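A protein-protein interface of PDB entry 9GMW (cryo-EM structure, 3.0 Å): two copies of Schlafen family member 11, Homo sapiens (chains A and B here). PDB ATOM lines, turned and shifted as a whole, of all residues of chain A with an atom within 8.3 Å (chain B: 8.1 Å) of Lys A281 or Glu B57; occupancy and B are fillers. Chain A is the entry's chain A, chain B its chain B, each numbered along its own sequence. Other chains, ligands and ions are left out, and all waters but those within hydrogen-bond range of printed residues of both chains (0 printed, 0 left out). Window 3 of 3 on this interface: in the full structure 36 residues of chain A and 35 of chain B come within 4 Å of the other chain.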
ATOM      1  N   ILE A 232      26.737  -9.062 -29.525  1.00  0.00           N
ATOM      2  CA  ILE A 232      25.706  -9.987 -29.065  1.00  0.00           C
ATOM      3  C   ILE A 232      24.705 -10.175 -30.200  1.00  0.00           C
ATOM      4  O   ILE A 232      23.978  -9.246 -30.557  1.00  0.00           O
ATOM      5  CB  ILE A 232      25.011  -9.471 -27.800  1.00  0.00           C
ATOM      6  CG1 ILE A 232      26.024  -9.222 -26.680  1.00  0.00           C
ATOM      7  CG2 ILE A 232      23.944 -10.456 -27.348  1.00  0.00           C
ATOM      8  CD1 ILE A 232      26.421 -10.459 -25.920  1.00  0.00           C
ATOM      9  N   PHE A 235      19.508 -13.224 -31.768  1.00  0.00           N
ATOM     10  CA  PHE A 235      18.629 -14.383 -31.826  1.00  0.00           C
ATOM     11  C   PHE A 235      19.267 -15.554 -31.098  1.00  0.00           C
ATOM     12  O   PHE A 235      20.495 -15.614 -30.971  1.00  0.00           O
ATOM     13  CB  PHE A 235      18.324 -14.784 -33.276  1.00  0.00           C
ATOM     14  CG  PHE A 235      19.515 -14.721 -34.181  1.00  0.00           C
ATOM     15  CD1 PHE A 235      20.394 -15.782 -34.265  1.00  0.00           C
ATOM     16  CD2 PHE A 235      19.759 -13.597 -34.945  1.00  0.00           C
ATOM     17  CE1 PHE A 235      21.488 -15.722 -35.093  1.00  0.00           C
ATOM     18  CE2 PHE A 235      20.855 -13.533 -35.774  1.00  0.00           C
ATOM     19  CZ  PHE A 235      21.720 -14.596 -35.847  1.00  0.00           C
ATOM     20  N   PRO A 236      18.466 -16.493 -30.608  1.00  0.00           N
ATOM     21  CA  PRO A 236      19.017 -17.667 -29.929  1.00  0.00           C
ATOM     22  C   PRO A 236      19.234 -18.822 -30.896  1.00  0.00           C
ATOM     23  O   PRO A 236      18.862 -18.773 -32.068  1.00  0.00           O
ATOM     24  CB  PRO A 236      17.929 -18.003 -28.911  1.00  0.00           C
ATOM     25  CG  PRO A 236      16.674 -17.664 -29.641  1.00  0.00           C
ATOM     26  CD  PRO A 236      16.996 -16.463 -30.511  1.00  0.00           C
ATOM     27  N   GLU A 237      19.850 -19.880 -30.376  1.00  0.00           N
ATOM     28  CA  GLU A 237      19.896 -21.132 -31.112  1.00  0.00           C
ATOM     29  C   GLU A 237      18.489 -21.697 -31.250  1.00  0.00           C
ATOM     30  O   GLU A 237      17.688 -21.664 -30.314  1.00  0.00           O
ATOM     31  CB  GLU A 237      20.792 -22.142 -30.400  1.00  0.00           C
ATOM     32  CG  GLU A 237      22.265 -21.824 -30.459  1.00  0.00           C
ATOM     33  CD  GLU A 237      23.111 -22.970 -29.961  1.00  0.00           C
ATOM     34  OE1 GLU A 237      22.610 -23.754 -29.133  1.00  0.00           O
ATOM     35  OE2 GLU A 237      24.276 -23.088 -30.392  1.00  0.00           O
ATOM     36  N   PHE A 243      25.235 -22.246 -32.671  1.00  0.00           N
ATOM     37  CA  PHE A 243      26.398 -21.443 -32.320  1.00  0.00           C
ATOM     38  C   PHE A 243      27.503 -22.346 -31.793  1.00  0.00           C
ATOM     39  O   PHE A 243      27.262 -23.173 -30.907  1.00  0.00           O
ATOM     40  CB  PHE A 243      26.051 -20.395 -31.261  1.00  0.00           C
ATOM     41  CG  PHE A 243      25.030 -19.391 -31.700  1.00  0.00           C
ATOM     42  CD1 PHE A 243      24.958 -18.975 -33.013  1.00  0.00           C
ATOM     43  CD2 PHE A 243      24.146 -18.853 -30.786  1.00  0.00           C
ATOM     44  CE1 PHE A 243      24.021 -18.050 -33.405  1.00  0.00           C
ATOM     45  CE2 PHE A 243      23.210 -17.929 -31.176  1.00  0.00           C
ATOM     46  CZ  PHE A 243      23.148 -17.527 -32.485  1.00  0.00           C
ATOM     47  N   LYS A 244      28.709 -22.176 -32.326  1.00  0.00           N
ATOM     48  CA  LYS A 244      29.870 -22.947 -31.909  1.00  0.00           C
ATOM     49  C   LYS A 244      31.066 -22.027 -31.727  1.00  0.00           C
ATOM     50  O   LYS A 244      31.278 -21.103 -32.517  1.00  0.00           O
ATOM     51  CB  LYS A 244      30.228 -24.034 -32.937  1.00  0.00           C
ATOM     52  CG  LYS A 244      29.303 -25.252 -33.016  1.00  0.00           C
ATOM     53  CD  LYS A 244      29.002 -25.892 -31.671  1.00  0.00           C
ATOM     54  CE  LYS A 244      29.686 -27.233 -31.542  1.00  0.00           C
ATOM     55  NZ  LYS A 244      29.183 -28.008 -30.379  1.00  0.00           N
ATOM     56  N   GLN A 245      31.847 -22.289 -30.685  1.00  0.00           N
ATOM     57  CA  GLN A 245      33.126 -21.621 -30.520  1.00  0.00           C
ATOM     58  C   GLN A 245      34.231 -22.418 -31.206  1.00  0.00           C
ATOM     59  O   GLN A 245      34.073 -23.596 -31.535  1.00  0.00           O
ATOM     60  CB  GLN A 245      33.468 -21.459 -29.042  1.00  0.00           C
ATOM     61  CG  GLN A 245      32.588 -20.495 -28.282  1.00  0.00           C
ATOM     62  CD  GLN A 245      33.305 -19.874 -27.105  1.00  0.00           C
ATOM     63  OE1 GLN A 245      34.507 -19.623 -27.158  1.00  0.00           O
ATOM     64  NE2 GLN A 245      32.573 -19.636 -26.025  1.00  0.00           N
ATOM     65  N   VAL A 278      31.044 -18.177 -32.300  1.00  0.00           N
ATOM     66  CA  VAL A 278      30.020 -17.464 -31.551  1.00  0.00           C
ATOM     67  C   VAL A 278      29.792 -18.206 -30.245  1.00  0.00           C
ATOM     68  O   VAL A 278      29.557 -19.418 -30.249  1.00  0.00           O
ATOM     69  CB  VAL A 278      28.709 -17.356 -32.352  1.00  0.00           C
ATOM     70  CG1 VAL A 278      27.648 -16.631 -31.547  1.00  0.00           C
ATOM     71  CG2 VAL A 278      28.957 -16.655 -33.673  1.00  0.00           C
ATOM     72  N   ASP A 279      29.856 -17.483 -29.131  1.00  0.00           N
ATOM     73  CA  ASP A 279      29.677 -18.101 -27.825  1.00  0.00           C
ATOM     74  C   ASP A 279      28.283 -18.710 -27.738  1.00  0.00           C
ATOM     75  O   ASP A 279      27.292 -18.070 -28.102  1.00  0.00           O
ATOM     76  CB  ASP A 279      29.888 -17.069 -26.720  1.00  0.00           C
ATOM     77  CG  ASP A 279      29.788 -17.669 -25.329  1.00  0.00           C
ATOM     78  OD1 ASP A 279      29.345 -18.826 -25.200  1.00  0.00           O
ATOM     79  OD2 ASP A 279      30.160 -16.980 -24.358  1.00  0.00           O
ATOM     80  N   ASP A 280      28.209 -19.949 -27.250  1.00  0.00           N
ATOM     81  CA  ASP A 280      26.933 -20.653 -27.203  1.00  0.00           C
ATOM     82  C   ASP A 280      26.018 -20.091 -26.124  1.00  0.00           C
ATOM     83  O   ASP A 280      24.795 -20.247 -26.207  1.00  0.00           O
ATOM     84  CB  ASP A 280      27.178 -22.142 -26.968  1.00  0.00           C
ATOM     85  CG  ASP A 280      25.912 -22.962 -27.043  1.00  0.00           C
ATOM     86  OD1 ASP A 280      25.249 -23.126 -25.999  1.00  0.00           O
ATOM     87  OD2 ASP A 280      25.590 -23.461 -28.142  1.00  0.00           O
ATOM     88  N   LYS A 281      26.585 -19.440 -25.107  1.00  0.00           N
ATOM     89  CA  LYS A 281      25.823 -18.977 -23.950  1.00  0.00           C
ATOM     90  C   LYS A 281      25.481 -17.494 -24.043  1.00  0.00           C
ATOM     91  O   LYS A 281      24.311 -17.116 -23.960  1.00  0.00           O
ATOM     92  CB  LYS A 281      26.612 -19.266 -22.667  1.00  0.00           C
ATOM     93  CG  LYS A 281      26.811 -20.744 -22.397  1.00  0.00           C
ATOM     94  CD  LYS A 281      27.457 -20.995 -21.047  1.00  0.00           C
ATOM     95  CE  LYS A 281      28.005 -22.413 -20.953  1.00  0.00           C
ATOM     96  NZ  LYS A 281      27.830 -23.003 -19.596  1.00  0.00           N
ATOM     97  N   SER A 282      26.489 -16.641 -24.207  1.00  0.00           N
ATOM     98  CA  SER A 282      26.267 -15.205 -24.284  1.00  0.00           C
ATOM     99  C   SER A 282      25.902 -14.734 -25.682  1.00  0.00           C
ATOM    100  O   SER A 282      25.544 -13.563 -25.846  1.00  0.00           O
ATOM    101  CB  SER A 282      27.514 -14.455 -23.819  1.00  0.00           C
ATOM    102  OG  SER A 282      28.546 -14.543 -24.785  1.00  0.00           O
ATOM    103  N   ARG A 283      25.989 -15.601 -26.686  1.00  0.00           N
ATOM    104  CA  ARG A 283      25.708 -15.243 -28.073  1.00  0.00           C
ATOM    105  C   ARG A 283      26.673 -14.186 -28.596  1.00  0.00           C
ATOM    106  O   ARG A 283      26.383 -13.518 -29.592  1.00  0.00           O
ATOM    107  CB  ARG A 283      24.261 -14.764 -28.238  1.00  0.00           C
ATOM    108  CG  ARG A 283      23.235 -15.664 -27.566  1.00  0.00           C
ATOM    109  CD  ARG A 283      21.865 -15.013 -27.505  1.00  0.00           C
ATOM    110  NE  ARG A 283      20.951 -15.759 -26.649  1.00  0.00           N
ATOM    111  CZ  ARG A 283      19.628 -15.670 -26.700  1.00  0.00           C
ATOM    112  NH1 ARG A 283      19.020 -14.865 -27.555  1.00  0.00           N
ATOM    113  NH2 ARG A 283      18.897 -16.408 -25.869  1.00  0.00           N
ATOM    114  N   GLU A 284      27.817 -14.024 -27.940  1.00  0.00           N
ATOM    115  CA  GLU A 284      28.814 -13.064 -28.388  1.00  0.00           C
ATOM    116  C   GLU A 284      29.579 -13.608 -29.584  1.00  0.00           C
ATOM    117  O   GLU A 284      29.787 -14.816 -29.711  1.00  0.00           O
ATOM    118  CB  GLU A 284      29.793 -12.748 -27.261  1.00  0.00           C
ATOM    119  CG  GLU A 284      29.403 -11.570 -26.404  1.00  0.00           C
ATOM    120  CD  GLU A 284      30.583 -10.964 -25.679  1.00  0.00           C
ATOM    121  OE1 GLU A 284      31.203 -11.669 -24.856  1.00  0.00           O
ATOM    122  OE2 GLU A 284      30.889  -9.780 -25.929  1.00  0.00           O
ATOM    123  N   LEU A 286      33.041 -14.167 -31.115  1.00  0.00           N
ATOM    124  CA  LEU A 286      34.422 -14.275 -30.665  1.00  0.00           C
ATOM    125  C   LEU A 286      35.403 -14.570 -31.786  1.00  0.00           C
ATOM    126  O   LEU A 286      36.472 -13.961 -31.824  1.00  0.00           O
ATOM    127  CB  LEU A 286      34.549 -15.374 -29.601  1.00  0.00           C
ATOM    128  CG  LEU A 286      33.663 -15.209 -28.367  1.00  0.00           C
ATOM    129  CD1 LEU A 286      33.815 -16.401 -27.445  1.00  0.00           C
ATOM    130  CD2 LEU A 286      33.982 -13.922 -27.630  1.00  0.00           C
ATOM    131  N   THR B  53      10.050 -20.486 -16.737  1.00  0.00           N
ATOM    132  CA  THR B  53      11.400 -20.022 -17.024  1.00  0.00           C
ATOM    133  C   THR B  53      11.870 -20.645 -18.329  1.00  0.00           C
ATOM    134  O   THR B  53      11.931 -21.873 -18.450  1.00  0.00           O
ATOM    135  CB  THR B  53      12.349 -20.387 -15.888  1.00  0.00           C
ATOM    136  OG1 THR B  53      11.726 -20.111 -14.629  1.00  0.00           O
ATOM    137  CG2 THR B  53      13.632 -19.595 -15.996  1.00  0.00           C
ATOM    138  N   LEU B  54      12.207 -19.806 -19.301  1.00  0.00           N
ATOM    139  CA  LEU B  54      12.601 -20.263 -20.621  1.00  0.00           C
ATOM    140  C   LEU B  54      14.035 -19.844 -20.900  1.00  0.00           C
ATOM    141  O   LEU B  54      14.489 -18.787 -20.457  1.00  0.00           O
ATOM    142  CB  LEU B  54      11.669 -19.706 -21.699  1.00  0.00           C
ATOM    143  CG  LEU B  54      10.224 -20.192 -21.597  1.00  0.00           C
ATOM    144  CD1 LEU B  54       9.367 -19.453 -22.582  1.00  0.00           C
ATOM    145  CD2 LEU B  54      10.125 -21.688 -21.832  1.00  0.00           C
ATOM    146  N   GLY B  55      14.741 -20.688 -21.643  1.00  0.00           N
ATOM    147  CA  GLY B  55      16.159 -20.507 -21.859  1.00  0.00           C
ATOM    148  C   GLY B  55      16.953 -21.547 -21.100  1.00  0.00           C
ATOM    149  O   GLY B  55      16.675 -21.814 -19.928  1.00  0.00           O
ATOM    150  N   GLU B  56      17.942 -22.147 -21.760  1.00  0.00           N
ATOM    151  CA  GLU B  56      18.708 -23.212 -21.125  1.00  0.00           C
ATOM    152  C   GLU B  56      19.456 -22.697 -19.902  1.00  0.00           C
ATOM    153  O   GLU B  56      19.426 -23.322 -18.837  1.00  0.00           O
ATOM    154  CB  GLU B  56      19.676 -23.824 -22.138  1.00  0.00           C
ATOM    155  CG  GLU B  56      20.579 -24.909 -21.573  1.00  0.00           C
ATOM    156  CD  GLU B  56      19.813 -25.983 -20.832  1.00  0.00           C
ATOM    157  OE1 GLU B  56      18.614 -26.166 -21.118  1.00  0.00           O
ATOM    158  OE2 GLU B  56      20.411 -26.645 -19.959  1.00  0.00           O
ATOM    159  N   GLU B  57      20.129 -21.552 -20.032  1.00  0.00           N
ATOM    160  CA  GLU B  57      20.882 -21.008 -18.907  1.00  0.00           C
ATOM    161  C   GLU B  57      19.960 -20.635 -17.756  1.00  0.00           C
ATOM    162  O   GLU B  57      20.240 -20.956 -16.592  1.00  0.00           O
ATOM    163  CB  GLU B  57      21.686 -19.792 -19.362  1.00  0.00           C
ATOM    164  CG  GLU B  57      22.936 -20.138 -20.151  1.00  0.00           C
ATOM    165  CD  GLU B  57      24.085 -20.573 -19.263  1.00  0.00           C
ATOM    166  OE1 GLU B  57      24.736 -19.695 -18.658  1.00  0.00           O
ATOM    167  OE2 GLU B  57      24.336 -21.792 -19.171  1.00  0.00           O
ATOM    168  N   ASN B  58      18.849 -19.963 -18.060  1.00  0.00           N
ATOM    169  CA  ASN B  58      17.921 -19.559 -17.010  1.00  0.00           C
ATOM    170  C   ASN B  58      17.359 -20.770 -16.283  1.00  0.00           C
ATOM    171  O   ASN B  58      17.245 -20.765 -15.053  1.00  0.00           O
ATOM    172  CB  ASN B  58      16.794 -18.721 -17.609  1.00  0.00           C
ATOM    173  CG  ASN B  58      17.297 -17.449 -18.253  1.00  0.00           C
ATOM    174  OD1 ASN B  58      18.252 -16.838 -17.781  1.00  0.00           O
ATOM    175  ND2 ASN B  58      16.655 -17.043 -19.340  1.00  0.00           N
ATOM    176  N   ARG B  59      16.998 -21.818 -17.025  1.00  0.00           N
ATOM    177  CA  ARG B  59      16.460 -23.011 -16.387  1.00  0.00           C
ATOM    178  C   ARG B  59      17.522 -23.739 -15.575  1.00  0.00           C
ATOM    179  O   ARG B  59      17.211 -24.310 -14.526  1.00  0.00           O
ATOM    180  CB  ARG B  59      15.856 -23.938 -17.439  1.00  0.00           C
ATOM    181  CG  ARG B  59      14.572 -23.400 -18.046  1.00  0.00           C
ATOM    182  CD  ARG B  59      13.847 -24.444 -18.873  1.00  0.00           C
ATOM    183  NE  ARG B  59      13.383 -25.567 -18.068  1.00  0.00           N
ATOM    184  CZ  ARG B  59      12.414 -25.502 -17.165  1.00  0.00           C
ATOM    185  NH1 ARG B  59      11.777 -24.372 -16.912  1.00  0.00           N
ATOM    186  NH2 ARG B  59      12.071 -26.601 -16.502  1.00  0.00           N
ATOM    187  N   LYS B  60      18.775 -23.737 -16.041  1.00  0.00           N
ATOM    188  CA  LYS B  60      19.851 -24.338 -15.261  1.00  0.00           C
ATOM    189  C   LYS B  60      20.077 -23.595 -13.953  1.00  0.00           C
ATOM    190  O   LYS B  60      20.321 -24.226 -12.918  1.00  0.00           O
ATOM    191  CB  LYS B  60      21.144 -24.360 -16.074  1.00  0.00           C
ATOM    192  CG  LYS B  60      21.268 -25.545 -17.018  1.00  0.00           C
ATOM    193  CD  LYS B  60      22.641 -25.634 -17.693  1.00  0.00           C
ATOM    194  CE  LYS B  60      23.377 -24.298 -17.756  1.00  0.00           C
ATOM    195  NZ  LYS B  60      24.469 -24.311 -18.767  1.00  0.00           N
ATOM    196  N   LYS B  61      20.002 -22.264 -13.974  1.00  0.00           N
ATOM    197  CA  LYS B  61      20.186 -21.489 -12.754  1.00  0.00           C
ATOM    198  C   LYS B  61      19.072 -21.709 -11.739  1.00  0.00           C
ATOM    199  O   LYS B  61      19.221 -21.291 -10.587  1.00  0.00           O
ATOM    200  CB  LYS B  61      20.279 -20.002 -13.085  1.00  0.00           C
ATOM    201  CG  LYS B  61      21.578 -19.596 -13.755  1.00  0.00           C
ATOM    202  CD  LYS B  61      21.490 -18.207 -14.378  1.00  0.00           C
ATOM    203  CE  LYS B  61      21.013 -17.161 -13.381  1.00  0.00           C
ATOM    204  NZ  LYS B  61      19.528 -17.104 -13.271  1.00  0.00           N
ATOM    205  N   LEU B  62      17.969 -22.339 -12.132  1.00  0.00           N
ATOM    206  CA  LEU B  62      16.883 -22.603 -11.203  1.00  0.00           C
ATOM    207  C   LEU B  62      17.269 -23.697 -10.220  1.00  0.00           C
ATOM    208  O   LEU B  62      18.288 -24.376 -10.365  1.00  0.00           O
ATOM    209  CB  LEU B  62      15.622 -23.044 -11.945  1.00  0.00           C
ATOM    210  CG  LEU B  62      14.868 -22.025 -12.791  1.00  0.00           C
ATOM    211  CD1 LEU B  62      13.738 -22.725 -13.516  1.00  0.00           C
ATOM    212  CD2 LEU B  62      14.337 -20.901 -11.927  1.00  0.00           C
ATOM    213  N   ARG B  67      12.351 -26.237 -11.411  1.00  0.00           N
ATOM    214  CA  ARG B  67      12.543 -26.690 -12.782  1.00  0.00           C
ATOM    215  C   ARG B  67      11.601 -27.842 -13.109  1.00  0.00           C
ATOM    216  O   ARG B  67      10.894 -27.819 -14.124  1.00  0.00           O
ATOM    217  CB  ARG B  67      14.000 -27.105 -12.978  1.00  0.00           C
ATOM    218  CG  ARG B  67      14.476 -27.091 -14.410  1.00  0.00           C
ATOM    219  CD  ARG B  67      15.835 -27.747 -14.526  1.00  0.00           C
ATOM    220  NE  ARG B  67      16.853 -27.031 -13.765  1.00  0.00           N
ATOM    221  CZ  ARG B  67      17.792 -27.604 -13.023  1.00  0.00           C
ATOM    222  NH1 ARG B  67      17.868 -28.918 -12.891  1.00  0.00           N
ATOM    223  NH2 ARG B  67      18.679 -26.838 -12.397  1.00  0.00           N
ATOM    224  N   HIS B  97      13.218 -10.501 -24.652  1.00  0.00           N
ATOM    225  CA  HIS B  97      13.902 -10.924 -25.861  1.00  0.00           C
ATOM    226  C   HIS B  97      13.621 -12.394 -26.161  1.00  0.00           C
ATOM    227  O   HIS B  97      13.247 -13.160 -25.270  1.00  0.00           O
ATOM    228  CB  HIS B  97      15.403 -10.701 -25.720  1.00  0.00           C
ATOM    229  CG  HIS B  97      16.066 -11.643 -24.764  1.00  0.00           C
ATOM    230  ND1 HIS B  97      15.611 -11.842 -23.479  1.00  0.00           N
ATOM    231  CD2 HIS B  97      17.153 -12.438 -24.905  1.00  0.00           C
ATOM    232  CE1 HIS B  97      16.387 -12.720 -22.871  1.00  0.00           C
ATOM    233  NE2 HIS B  97      17.331 -13.098 -23.713  1.00  0.00           N
ATOM    234  N   GLU B 100      15.367 -19.573 -26.323  1.00  0.00           N
ATOM    235  CA  GLU B 100      15.121 -20.968 -26.649  1.00  0.00           C
ATOM    236  C   GLU B 100      14.306 -21.675 -25.568  1.00  0.00           C
ATOM    237  O   GLU B 100      14.250 -21.250 -24.413  1.00  0.00           O
ATOM    238  CB  GLU B 100      16.442 -21.710 -26.877  1.00  0.00           C
ATOM    239  CG  GLU B 100      17.293 -21.944 -25.627  1.00  0.00           C
ATOM    240  CD  GLU B 100      17.999 -20.690 -25.142  1.00  0.00           C
ATOM    241  OE1 GLU B 100      17.987 -19.675 -25.868  1.00  0.00           O
ATOM    242  OE2 GLU B 100      18.564 -20.716 -24.029  1.00  0.00           O
ATOM    243  N   MET B 101      13.664 -22.772 -25.961  1.00  0.00           N
ATOM    244  CA  MET B 101      12.796 -23.490 -25.034  1.00  0.00           C
ATOM    245  C   MET B 101      13.576 -23.965 -23.813  1.00  0.00           C
ATOM    246  O   MET B 101      13.226 -23.639 -22.675  1.00  0.00           O
ATOM    247  CB  MET B 101      12.130 -24.660 -25.754  1.00  0.00           C
ATOM    248  CG  MET B 101      11.136 -25.426 -24.900  1.00  0.00           C
ATOM    249  SD  MET B 101      10.244 -26.748 -25.751  1.00  0.00           S
ATOM    250  CE  MET B 101       9.002 -25.852 -26.677  1.00  0.00           C
ATOM    251  N   GLY B 102      14.644 -24.724 -24.032  1.00  0.00           N
ATOM    252  CA  GLY B 102      15.375 -25.337 -22.941  1.00  0.00           C
ATOM    253  C   GLY B 102      15.541 -26.818 -23.204  1.00  0.00           C
ATOM    254  O   GLY B 102      14.623 -27.473 -23.708  1.00  0.00           O
ATOM    255  N   LEU B 103      16.709 -27.362 -22.859  1.00  0.00           N
ATOM    256  CA  LEU B 103      17.017 -28.738 -23.229  1.00  0.00           C
ATOM    257  C   LEU B 103      16.109 -29.742 -22.532  1.00  0.00           C
ATOM    258  O   LEU B 103      15.716 -30.737 -23.146  1.00  0.00           O
ATOM    259  CB  LEU B 103      18.480 -29.049 -22.924  1.00  0.00           C
ATOM    260  CG  LEU B 103      19.508 -28.299 -23.771  1.00  0.00           C
ATOM    261  CD1 LEU B 103      20.913 -28.696 -23.364  1.00  0.00           C
ATOM    262  CD2 LEU B 103      19.293 -28.551 -25.252  1.00  0.00           C
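Among the printed residues, merely in contact across the chains: Pro A236 with Glu B100 (3.5 Å), Glu A237 with Glu B100 (3.7 Å) and Lys A281 with Lys B60 (3.7 Å).
Of the 16 printed residues of chain B, 3 touch a printed residue of chain A.
Printed residues of chain B that touch a printed residue of chain A: Glu B57, Lys B60 and Glu B100.
Among the printed residues, Asp or Glu carboxylates within 4 Å of a Lys or Arg side-chain nitrogen of the other chain: Lys A281 with Glu B57 (3.7 Å) and Arg A283 with Glu B100 (3.4 Å).
NZ of Lys A281 is in salt-bridge range of OE2 of Glu B57 (3.7 Å).
OE1 of Glu B100 lies within salt-bridge range of NH2 of Arg A283, 3.4 Å away.
No position is printed for both chains.
Of the 5 pairs that touch across the chains among the printed residues, none has its exchanged pair printed and touching as well.
Lys A281 touches just these residues of chain B: Glu B57 and Lys B60.
Of the printed residues of chain A, Lys B60 touches Lys A281 (3.7 Å).
Of the printed residues of chain B, Glu A237 touches Glu B100.
Of the printed residues of chain B, Arg A283 touches Glu B100.
Of the printed residues of chain B, Pro A236 touches Glu B100.
The nearest residue of chain B that does not touch Lys A281 is Glu B100 (6.8 Å).
The nearest residue of chain A that does not touch Glu B57 is Asp A280 (6.3 Å).
The side-chain amino group (NZ) of Lys B60 lies within salt-bridge range of the side-chain carboxylate (OE2) of Glu B57, at 2.6 Å.
The backbone NH of Lys A281 is in hydrogen-bond range of the side-chain carboxylate of Asp A279 (2.8 Å).
The backbone NH (N) of Gly B55 lies within hydrogen-bond range of the backbone carbonyl oxygen (O) of Glu B100.
OE2 of Glu B100 is in hydrogen-bond range of N of Glu B56, 2.8 Å away.
NH2 of Arg B67 is in hydrogen-bond range of O of Lys B60 (3.1 Å).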
